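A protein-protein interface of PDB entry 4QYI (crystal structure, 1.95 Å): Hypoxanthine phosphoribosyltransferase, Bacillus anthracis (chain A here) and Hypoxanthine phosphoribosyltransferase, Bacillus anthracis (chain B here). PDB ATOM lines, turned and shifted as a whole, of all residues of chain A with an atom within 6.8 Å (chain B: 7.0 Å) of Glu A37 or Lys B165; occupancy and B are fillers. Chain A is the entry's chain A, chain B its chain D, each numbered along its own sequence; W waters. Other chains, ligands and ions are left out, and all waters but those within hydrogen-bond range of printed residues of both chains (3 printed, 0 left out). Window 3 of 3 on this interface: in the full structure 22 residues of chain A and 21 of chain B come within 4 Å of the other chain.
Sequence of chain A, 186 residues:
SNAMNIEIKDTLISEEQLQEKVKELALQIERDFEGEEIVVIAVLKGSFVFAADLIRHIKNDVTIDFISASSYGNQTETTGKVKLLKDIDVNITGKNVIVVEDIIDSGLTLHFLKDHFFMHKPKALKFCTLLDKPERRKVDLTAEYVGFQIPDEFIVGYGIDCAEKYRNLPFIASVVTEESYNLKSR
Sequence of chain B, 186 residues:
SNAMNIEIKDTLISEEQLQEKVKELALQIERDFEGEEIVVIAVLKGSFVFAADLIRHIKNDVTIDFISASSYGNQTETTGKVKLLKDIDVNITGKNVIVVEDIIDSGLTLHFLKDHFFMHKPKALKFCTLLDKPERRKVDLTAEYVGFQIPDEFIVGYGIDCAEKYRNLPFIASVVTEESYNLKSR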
ATOM      1  N   PHE A  33       8.140 -18.102  -9.120  1.00  0.00           N
ATOM      2  CA  PHE A  33       9.268 -17.718  -8.277  1.00  0.00           C
ATOM      3  C   PHE A  33      10.061 -16.595  -8.875  1.00  0.00           C
ATOM      4  O   PHE A  33      11.301 -16.608  -8.868  1.00  0.00           O
ATOM      5  CB  PHE A  33      10.160 -18.945  -8.019  1.00  0.00           C
ATOM      6  CG  PHE A  33       9.443 -20.034  -7.294  1.00  0.00           C
ATOM      7  CD1 PHE A  33       9.287 -19.957  -5.925  1.00  0.00           C
ATOM      8  CD2 PHE A  33       8.882 -21.103  -7.975  1.00  0.00           C
ATOM      9  CE1 PHE A  33       8.601 -20.934  -5.252  1.00  0.00           C
ATOM     10  CE2 PHE A  33       8.185 -22.092  -7.300  1.00  0.00           C
ATOM     11  CZ  PHE A  33       8.040 -22.004  -5.932  1.00  0.00           C
ATOM     12  N   GLY A  35      12.097 -13.530  -9.482  1.00  0.00           N
ATOM     13  CA  GLY A  35      13.092 -12.855  -8.656  1.00  0.00           C
ATOM     14  C   GLY A  35      13.706 -13.653  -7.508  1.00  0.00           C
ATOM     15  O   GLY A  35      14.378 -13.074  -6.659  1.00  0.00           O
ATOM     16  N   GLU A  36      13.539 -14.973  -7.488  1.00  0.00           N
ATOM     17  CA  GLU A  36      14.105 -15.765  -6.398  1.00  0.00           C
ATOM     18  C   GLU A  36      14.903 -16.976  -6.830  1.00  0.00           C
ATOM     19  O   GLU A  36      14.734 -17.498  -7.920  1.00  0.00           O
ATOM     20  CB  GLU A  36      13.003 -16.242  -5.448  1.00  0.00           C
ATOM     21  CG  GLU A  36      12.144 -15.100  -4.928  1.00  0.00           C
ATOM     22  CD  GLU A  36      11.266 -15.474  -3.761  1.00  0.00           C
ATOM     23  OE1 GLU A  36      10.113 -15.017  -3.769  1.00  0.00           O
ATOM     24  OE2 GLU A  36      11.711 -16.213  -2.841  1.00  0.00           O
ATOM     25  N   GLU A  37      15.773 -17.411  -5.930  1.00  0.00           N
ATOM     26  CA  GLU A  37      16.580 -18.620  -6.103  1.00  0.00           C
ATOM     27  C   GLU A  37      15.667 -19.814  -5.827  1.00  0.00           C
ATOM     28  O   GLU A  37      14.682 -19.681  -5.105  1.00  0.00           O
ATOM     29  CB  GLU A  37      17.733 -18.636  -5.109  1.00  0.00           C
ATOM     30  CG  GLU A  37      18.614 -17.398  -5.202  1.00  0.00           C
ATOM     31  CD  GLU A  37      19.725 -17.401  -4.167  1.00  0.00           C
ATOM     32  OE1 GLU A  37      20.055 -18.484  -3.641  1.00  0.00           O
ATOM     33  OE2 GLU A  37      20.265 -16.312  -3.882  1.00  0.00           O
ATOM     34  N   ILE A  38      15.993 -20.966  -6.404  1.00  0.00           N
ATOM     35  CA  ILE A  38      15.209 -22.173  -6.223  1.00  0.00           C
ATOM     36  C   ILE A  38      16.108 -23.356  -5.947  1.00  0.00           C
ATOM     37  O   ILE A  38      17.211 -23.433  -6.472  1.00  0.00           O
ATOM     38  CB  ILE A  38      14.427 -22.521  -7.505  1.00  0.00           C
ATOM     39  CG1 ILE A  38      13.481 -21.381  -7.880  1.00  0.00           C
ATOM     40  CG2 ILE A  38      13.623 -23.801  -7.323  1.00  0.00           C
ATOM     41  CD1 ILE A  38      12.893 -21.545  -9.267  1.00  0.00           C
ATOM     42  N   VAL A  39      15.634 -24.271  -5.097  1.00  0.00           N
ATOM     43  CA  VAL A  39      16.338 -25.510  -4.839  1.00  0.00           C
ATOM     44  C   VAL A  39      15.474 -26.603  -5.477  1.00  0.00           C
ATOM     45  O   VAL A  39      14.280 -26.723  -5.184  1.00  0.00           O
ATOM     46  CB  VAL A  39      16.507 -25.831  -3.341  1.00  0.00           C
ATOM     47  CG1 VAL A  39      17.128 -27.221  -3.156  1.00  0.00           C
ATOM     48  CG2 VAL A  39      17.349 -24.761  -2.655  1.00  0.00           C
ATOM     49  N   ASN A  60      16.237 -18.873 -13.360  1.00  0.00           N
ATOM     50  CA  ASN A  60      16.527 -18.500 -11.984  1.00  0.00           C
ATOM     51  C   ASN A  60      17.792 -19.215 -11.506  1.00  0.00           C
ATOM     52  O   ASN A  60      18.230 -20.211 -12.111  1.00  0.00           O
ATOM     53  CB  ASN A  60      15.414 -18.953 -11.030  1.00  0.00           C
ATOM     54  CG  ASN A  60      14.048 -18.395 -11.381  1.00  0.00           C
ATOM     55  OD1 ASN A  60      13.548 -18.619 -12.479  1.00  0.00           O
ATOM     56  ND2 ASN A  60      13.395 -17.745 -10.416  1.00  0.00           N
ATOM     57  N   ASP A  61      18.386 -18.709 -10.421  1.00  0.00           N
ATOM     58  CA  ASP A  61      19.526 -19.395  -9.791  1.00  0.00           C
ATOM     59  C   ASP A  61      18.981 -20.684  -9.228  1.00  0.00           C
ATOM     60  O   ASP A  61      18.142 -20.659  -8.342  1.00  0.00           O
ATOM     61  CB  ASP A  61      20.145 -18.651  -8.584  1.00  0.00           C
ATOM     62  CG  ASP A  61      21.176 -17.621  -8.995  1.00  0.00           C
ATOM     63  OD1 ASP A  61      21.523 -17.557 -10.196  1.00  0.00           O
ATOM     64  OD2 ASP A  61      21.655 -16.882  -8.107  1.00  0.00           O
ATOM     65  N   VAL A  62      19.501 -21.808  -9.687  1.00  0.00           N
ATOM     66  CA  VAL A  62      19.045 -23.095  -9.207  1.00  0.00           C
ATOM     67  C   VAL A  62      20.134 -23.893  -8.497  1.00  0.00           C
ATOM     68  O   VAL A  62      21.264 -23.976  -8.969  1.00  0.00           O
ATOM     69  CB  VAL A  62      18.511 -23.937 -10.394  1.00  0.00           C
ATOM     70  CG1 VAL A  62      18.258 -25.378  -9.991  1.00  0.00           C
ATOM     71  CG2 VAL A  62      17.234 -23.329 -10.983  1.00  0.00           C
ATOM     72  N   THR A  63      19.765 -24.494  -7.373  1.00  0.00           N
ATOM     73  CA  THR A  63      20.633 -25.420  -6.634  1.00  0.00           C
ATOM     74  C   THR A  63      19.948 -26.767  -6.790  1.00  0.00           C
ATOM     75  O   THR A  63      18.737 -26.866  -6.620  1.00  0.00           O
ATOM     76  CB  THR A  63      20.732 -25.086  -5.144  1.00  0.00           C
ATOM     77  OG1 THR A  63      21.454 -23.880  -4.999  1.00  0.00           O
ATOM     78  CG2 THR A  63      21.483 -26.190  -4.349  1.00  0.00           C
ATOM     79  N   ILE A  64      20.672 -27.802  -7.183  1.00  0.00           N
ATOM     80  CA  ILE A  64      19.998 -29.093  -7.301  1.00  0.00           C
ATOM     81  C   ILE A  64      20.612 -30.110  -6.348  1.00  0.00           C
ATOM     82  O   ILE A  64      21.794 -30.082  -6.084  1.00  0.00           O
ATOM     83  CB  ILE A  64      19.885 -29.615  -8.758  1.00  0.00           C
ATOM     84  CG1 ILE A  64      19.075 -30.926  -8.797  1.00  0.00           C
ATOM     85  CG2 ILE A  64      21.247 -29.837  -9.366  1.00  0.00           C
ATOM     86  CD1 ILE A  64      18.552 -31.298 -10.170  1.00  0.00           C
ATOM     87  N   LYS A  95      14.221 -21.719   2.090  1.00  0.00           N
ATOM     88  CA  LYS A  95      14.368 -21.700   0.641  1.00  0.00           C
ATOM     89  C   LYS A  95      13.111 -22.142  -0.078  1.00  0.00           C
ATOM     90  O   LYS A  95      12.193 -22.722   0.512  1.00  0.00           O
ATOM     91  CB  LYS A  95      15.484 -22.644   0.211  1.00  0.00           C
ATOM     92  CG  LYS A  95      16.820 -22.430   0.904  1.00  0.00           C
ATOM     93  CD  LYS A  95      17.402 -21.065   0.662  1.00  0.00           C
ATOM     94  CE  LYS A  95      18.690 -20.909   1.452  1.00  0.00           C
ATOM     95  NZ  LYS A  95      19.202 -19.519   1.373  1.00  0.00           N
ATOM     96  N   ASN A  96      13.091 -21.836  -1.369  1.00  0.00           N
ATOM     97  CA  ASN A  96      12.018 -22.268  -2.255  1.00  0.00           C
ATOM     98  C   ASN A  96      12.435 -23.621  -2.784  1.00  0.00           C
ATOM     99  O   ASN A  96      13.476 -23.739  -3.422  1.00  0.00           O
ATOM    100  CB  ASN A  96      11.884 -21.300  -3.395  1.00  0.00           C
ATOM    101  CG  ASN A  96      11.451 -19.941  -2.924  1.00  0.00           C
ATOM    102  OD1 ASN A  96      10.498 -19.825  -2.156  1.00  0.00           O
ATOM    103  ND2 ASN A  96      12.104 -18.911  -3.405  1.00  0.00           N
ATOM    104  N   VAL A  97      11.617 -24.635  -2.544  1.00  0.00           N
ATOM    105  CA  VAL A  97      11.964 -25.979  -2.964  1.00  0.00           C
ATOM    106  C   VAL A  97      10.958 -26.598  -3.924  1.00  0.00           C
ATOM    107  O   VAL A  97       9.738 -26.557  -3.702  1.00  0.00           O
ATOM    108  CB  VAL A  97      12.029 -26.913  -1.739  1.00  0.00           C
ATOM    109  CG1 VAL A  97      12.433 -28.317  -2.152  1.00  0.00           C
ATOM    110  CG2 VAL A  97      12.989 -26.373  -0.693  1.00  0.00           C
ATOM    111  N   ILE B   6      30.760 -14.767  -6.731  1.00  0.00           N
ATOM    112  CA  ILE B   6      30.946 -15.691  -7.884  1.00  0.00           C
ATOM    113  C   ILE B   6      30.115 -15.255  -9.079  1.00  0.00           C
ATOM    114  O   ILE B   6      28.882 -15.296  -9.042  1.00  0.00           O
ATOM    115  CB  ILE B   6      30.594 -17.134  -7.481  1.00  0.00           C
ATOM    116  CG1 ILE B   6      31.400 -17.430  -6.170  1.00  0.00           C
ATOM    117  CG2 ILE B   6      30.735 -18.079  -8.703  1.00  0.00           C
ATOM    118  CD1 ILE B   6      31.307 -18.838  -5.623  1.00  0.00           C
ATOM    119  N   VAL B 156      31.931 -23.895 -14.703  1.00  0.00           N
ATOM    120  CA  VAL B 156      30.613 -24.256 -14.198  1.00  0.00           C
ATOM    121  C   VAL B 156      29.685 -24.506 -15.377  1.00  0.00           C
ATOM    122  O   VAL B 156      30.024 -24.175 -16.524  1.00  0.00           O
ATOM    123  CB  VAL B 156      30.013 -23.130 -13.328  1.00  0.00           C
ATOM    124  CG1 VAL B 156      30.867 -22.873 -12.090  1.00  0.00           C
ATOM    125  CG2 VAL B 156      29.847 -21.846 -14.129  1.00  0.00           C
ATOM    126  N   GLY B 157      28.524 -25.084 -15.085  1.00  0.00           N
ATOM    127  CA  GLY B 157      27.506 -25.361 -16.094  1.00  0.00           C
ATOM    128  C   GLY B 157      27.397 -26.821 -16.512  1.00  0.00           C
ATOM    129  O   GLY B 157      28.284 -27.623 -16.238  1.00  0.00           O
ATOM    130  N   GLY B 159      25.742 -29.355 -15.404  1.00  0.00           N
ATOM    131  CA  GLY B 159      25.905 -30.270 -14.264  1.00  0.00           C
ATOM    132  C   GLY B 159      27.001 -29.935 -13.254  1.00  0.00           C
ATOM    133  O   GLY B 159      26.949 -30.371 -12.107  1.00  0.00           O
ATOM    134  N   ILE B 160      27.974 -29.139 -13.676  1.00  0.00           N
ATOM    135  CA  ILE B 160      29.130 -28.753 -12.855  1.00  0.00           C
ATOM    136  C   ILE B 160      28.841 -27.473 -12.066  1.00  0.00           C
ATOM    137  O   ILE B 160      28.401 -26.456 -12.618  1.00  0.00           O
ATOM    138  CB  ILE B 160      30.355 -28.525 -13.774  1.00  0.00           C
ATOM    139  CG1 ILE B 160      30.523 -29.737 -14.681  1.00  0.00           C
ATOM    140  CG2 ILE B 160      31.632 -28.262 -12.973  1.00  0.00           C
ATOM    141  CD1 ILE B 160      31.538 -29.561 -15.780  1.00  0.00           C
ATOM    142  N   ASP B 161      29.131 -27.508 -10.773  1.00  0.00           N
ATOM    143  CA  ASP B 161      28.853 -26.366  -9.919  1.00  0.00           C
ATOM    144  C   ASP B 161      30.061 -25.612  -9.385  1.00  0.00           C
ATOM    145  O   ASP B 161      31.203 -26.000  -9.579  1.00  0.00           O
ATOM    146  CB  ASP B 161      28.160 -26.857  -8.642  1.00  0.00           C
ATOM    147  CG  ASP B 161      29.112 -27.613  -7.722  1.00  0.00           C
ATOM    148  OD1 ASP B 161      29.786 -28.552  -8.190  1.00  0.00           O
ATOM    149  OD2 ASP B 161      29.174 -27.301  -6.515  1.00  0.00           O
ATOM    150  N   CME B 162      29.735 -24.523  -8.691  1.00  0.00           N
ATOM    151  CA  CME B 162      30.671 -23.726  -7.923  1.00  0.00           C
ATOM    152  CB  CME B 162      31.095 -22.405  -8.544  1.00  0.00           C
ATOM    153  SG  CME B 162      32.029 -21.490  -7.362  1.00  0.00           S
ATOM    154  SD  CME B 162      33.763 -22.468  -7.271  1.00  0.00           S
ATOM    155  CE  CME B 162      34.732 -21.002  -7.028  1.00  0.00           C
ATOM    156  CZ  CME B 162      36.070 -21.068  -7.713  1.00  0.00           C
ATOM    157  OH  CME B 162      37.067 -21.202  -6.703  1.00  0.00           O
ATOM    158  C   CME B 162      29.838 -23.513  -6.679  1.00  0.00           C
ATOM    159  O   CME B 162      28.843 -22.797  -6.717  1.00  0.00           O
ATOM    160  N   ALA B 163      30.217 -24.167  -5.581  1.00  0.00           N
ATOM    161  CA  ALA B 163      29.495 -24.072  -4.312  1.00  0.00           C
ATOM    162  C   ALA B 163      28.006 -24.382  -4.501  1.00  0.00           C
ATOM    163  O   ALA B 163      27.136 -23.674  -4.001  1.00  0.00           O
ATOM    164  CB  ALA B 163      29.705 -22.708  -3.659  1.00  0.00           C
ATOM    165  N   GLU B 164      27.736 -25.440  -5.260  1.00  0.00           N
ATOM    166  CA  GLU B 164      26.376 -25.938  -5.546  1.00  0.00           C
ATOM    167  C   GLU B 164      25.546 -25.070  -6.485  1.00  0.00           C
ATOM    168  O   GLU B 164      24.381 -25.364  -6.744  1.00  0.00           O
ATOM    169  CB  GLU B 164      25.602 -26.234  -4.247  1.00  0.00           C
ATOM    170  CG  GLU B 164      26.274 -27.266  -3.339  1.00  0.00           C
ATOM    171  CD  GLU B 164      26.495 -28.623  -4.007  1.00  0.00           C
ATOM    172  OE1 GLU B 164      25.793 -28.960  -4.983  1.00  0.00           O
ATOM    173  OE2 GLU B 164      27.377 -29.374  -3.543  1.00  0.00           O
ATOM    174  N   LYS B 165      26.151 -24.019  -7.019  1.00  0.00           N
ATOM    175  CA  LYS B 165      25.457 -23.159  -7.964  1.00  0.00           C
ATOM    176  C   LYS B 165      25.897 -23.371  -9.419  1.00  0.00           C
ATOM    177  O   LYS B 165      26.970 -23.904  -9.687  1.00  0.00           O
ATOM    178  CB  LYS B 165      25.578 -21.697  -7.547  1.00  0.00           C
ATOM    179  CG  LYS B 165      24.450 -21.278  -6.629  1.00  0.00           C
ATOM    180  CD  LYS B 165      24.539 -19.801  -6.322  1.00  0.00           C
ATOM    181  CE  LYS B 165      23.425 -19.388  -5.388  1.00  0.00           C
ATOM    182  NZ  LYS B 165      23.290 -17.917  -5.264  1.00  0.00           N
ATOM    183  N   TYR B 166      25.028 -22.958 -10.339  1.00  0.00           N
ATOM    184  CA  TYR B 166      25.262 -23.005 -11.790  1.00  0.00           C
ATOM    185  C   TYR B 166      25.197 -24.354 -12.505  1.00  0.00           C
ATOM    186  O   TYR B 166      25.514 -24.426 -13.681  1.00  0.00           O
ATOM    187  CB  TYR B 166      26.569 -22.308 -12.155  1.00  0.00           C
ATOM    188  CG  TYR B 166      26.631 -20.846 -11.760  1.00  0.00           C
ATOM    189  CD1 TYR B 166      25.730 -19.926 -12.285  1.00  0.00           C
ATOM    190  CD2 TYR B 166      27.648 -20.367 -10.928  1.00  0.00           C
ATOM    191  CE1 TYR B 166      25.813 -18.579 -11.950  1.00  0.00           C
ATOM    192  CE2 TYR B 166      27.746 -19.021 -10.595  1.00  0.00           C
ATOM    193  CZ  TYR B 166      26.829 -18.128 -11.103  1.00  0.00           C
ATOM    194  OH  TYR B 166      26.955 -16.784 -10.780  1.00  0.00           O
ATOM    195  N   ARG B 167      24.754 -25.408 -11.834  1.00  0.00           N
ATOM    196  CA  ARG B 167      24.661 -26.702 -12.489  1.00  0.00           C
ATOM    197  C   ARG B 167      23.642 -26.697 -13.601  1.00  0.00           C
ATOM    198  O   ARG B 167      23.717 -27.520 -14.509  1.00  0.00           O
ATOM    199  CB  ARG B 167      24.254 -27.805 -11.522  1.00  0.00           C
ATOM    200  CG  ARG B 167      25.230 -28.089 -10.405  1.00  0.00           C
ATOM    201  CD  ARG B 167      24.859 -29.402  -9.731  1.00  0.00           C
ATOM    202  NE  ARG B 167      25.582 -29.634  -8.501  1.00  0.00           N
ATOM    203  CZ  ARG B 167      26.759 -30.240  -8.393  1.00  0.00           C
ATOM    204  NH1 ARG B 167      27.417 -30.670  -9.456  1.00  0.00           N
ATOM    205  NH2 ARG B 167      27.294 -30.399  -7.190  1.00  0.00           N
ATOM    206  N   ASN B 168      22.705 -25.758 -13.561  1.00  0.00           N
ATOM    207  CA  ASN B 168      21.666 -25.726 -14.568  1.00  0.00           C
ATOM    208  C   ASN B 168      21.982 -24.979 -15.862  1.00  0.00           C
ATOM    209  O   ASN B 168      21.122 -24.889 -16.721  1.00  0.00           O
ATOM    210  CB  ASN B 168      20.409 -25.120 -13.992  1.00  0.00           C
ATOM    211  CG  ASN B 168      20.600 -23.685 -13.581  1.00  0.00           C
ATOM    212  OD1 ASN B 168      21.615 -23.327 -12.996  1.00  0.00           O
ATOM    213  ND2 ASN B 168      19.599 -22.867 -13.838  1.00  0.00           N
ATOM    214  N   LEU B 169      23.166 -24.399 -16.003  1.00  0.00           N
ATOM    215  CA  LEU B 169      23.462 -23.701 -17.251  1.00  0.00           C
ATOM    216  C   LEU B 169      23.521 -24.722 -18.372  1.00  0.00           C
ATOM    217  O   LEU B 169      24.084 -25.787 -18.197  1.00  0.00           O
ATOM    218  CB  LEU B 169      24.799 -22.961 -17.180  1.00  0.00           C
ATOM    219  CG  LEU B 169      24.958 -21.956 -16.046  1.00  0.00           C
ATOM    220  CD1 LEU B 169      26.335 -21.308 -16.122  1.00  0.00           C
ATOM    221  CD2 LEU B 169      23.873 -20.895 -16.095  1.00  0.00           C
HETATM  222  O   HOH W   1      23.867 -28.021  -7.056  1.00  0.00           O
HETATM  223  O   HOH W   2      23.158 -25.811  -9.370  1.00  0.00           O
HETATM  224  O   HOH W   3      22.837 -21.377 -10.455  1.00  0.00           O
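Of the printed residues of chain B, Glu A37 touches Lys B165.
Of chain A, only Glu A37 and Asp A61 come within 4 Å of Lys B165.
Of the printed residues of chain B, Asn A60 touches Asn B168.
Of the printed residues of chain A, Asn B168 touches Asn A60 (3.5 Å) and Val A62 (3.7 Å).
Of the printed residues of chain A, Glu B164 touches Thr A63.
Printed residues of chain B within 4 Å of Val A62: Asn B168 (3.7 Å).
Of the printed residues of chain B, Thr A63 touches Glu B164.
The nearest printed residue of chain B that does not touch Glu A37 is Glu B164 (8.7 Å).
The nearest residue of chain A that does not touch Lys B165 is Thr A63 (4.3 Å).
Printed residues of chain B that touch a printed residue of chain A: Glu B164, Lys B165, Arg B167 and Asn B168.
Of the 14 printed residues of chain A, 6 touch a printed residue of chain B.
Hydrophobic or aromatic side chains of chain A within 4 Å of the printed part of chain B: Val A62 and Ile A64.
Among the printed residues, 6 pairs touch across the chains.
Among the printed residues, Asp or Glu carboxylates within 4 Å of a Lys or Arg side-chain nitrogen of the other chain: Glu A37 with Lys B165 and Asp A61 with Lys B165.
Val A62 touches Asn B168 (CG2 to ND2, 3.7 Å).
Glu B164 touches Thr A63.
CG2 of Ile A64 touches CD of Arg B167, at 3.7 Å.
The backbone carbonyl oxygen (O) of Phe A33 is in hydrogen-bond range of the side-chain amide nitrogen (ND2) of Asn A60, at 2.8 Å.
The backbone carbonyl oxygen (O) of Glu A36 lies within hydrogen-bond range of the side-chain amide nitrogen (ND2) of Asn A60, at 2.8 Å.
The backbone NH (N) of Ile A38 lies within hydrogen-bond range of the backbone carbonyl oxygen (O) of Asp A61 (2.9 Å).
The backbone carbonyl oxygen of Gly B159 is in hydrogen-bond range of the guanidinium group of Arg B167 (2.7 Å).
OD2 of Asp B161 sits at hydrogen-bond distance from N of Glu B164 (2.7 Å).
The side-chain carboxylate (OE1) of Glu B164 lies within salt-bridge range of the guanidinium group (NH2) of Arg B167 (3.0 Å).
The side-chain amino group (NZ) of Lys B165 is in salt-bridge range of the side-chain carboxylate (OE1) of Glu A37 (3.7 Å).
The side-chain amide nitrogen (ND2) of Asn B168 is in hydrogen-bond range of the backbone carbonyl oxygen (O) of Asn A60 (3.5 Å).
OD2 of Asp A61 lies within salt-bridge range of NZ of Lys B165, at 3.4 Å.
Water W2 lies within hydrogen-bond range of O of Val A62 (2.7 Å), O of Glu B164 (2.9 Å) and N of Arg B167 (3.0 Å).
Water W3 lies within hydrogen-bond range of N of Tyr B166 (2.7 Å), O of Val A62 (3.4 Å) and OD1 of Asn B168 (3.4 Å).
Water W1 lies within hydrogen-bond range of the backbone carbonyl oxygen (O) of Glu B164 (2.7 Å), the guanidinium group (NE) of Arg B167 (2.8 Å) and the backbone carbonyl oxygen (O) of Ile A64 (3.1 Å).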
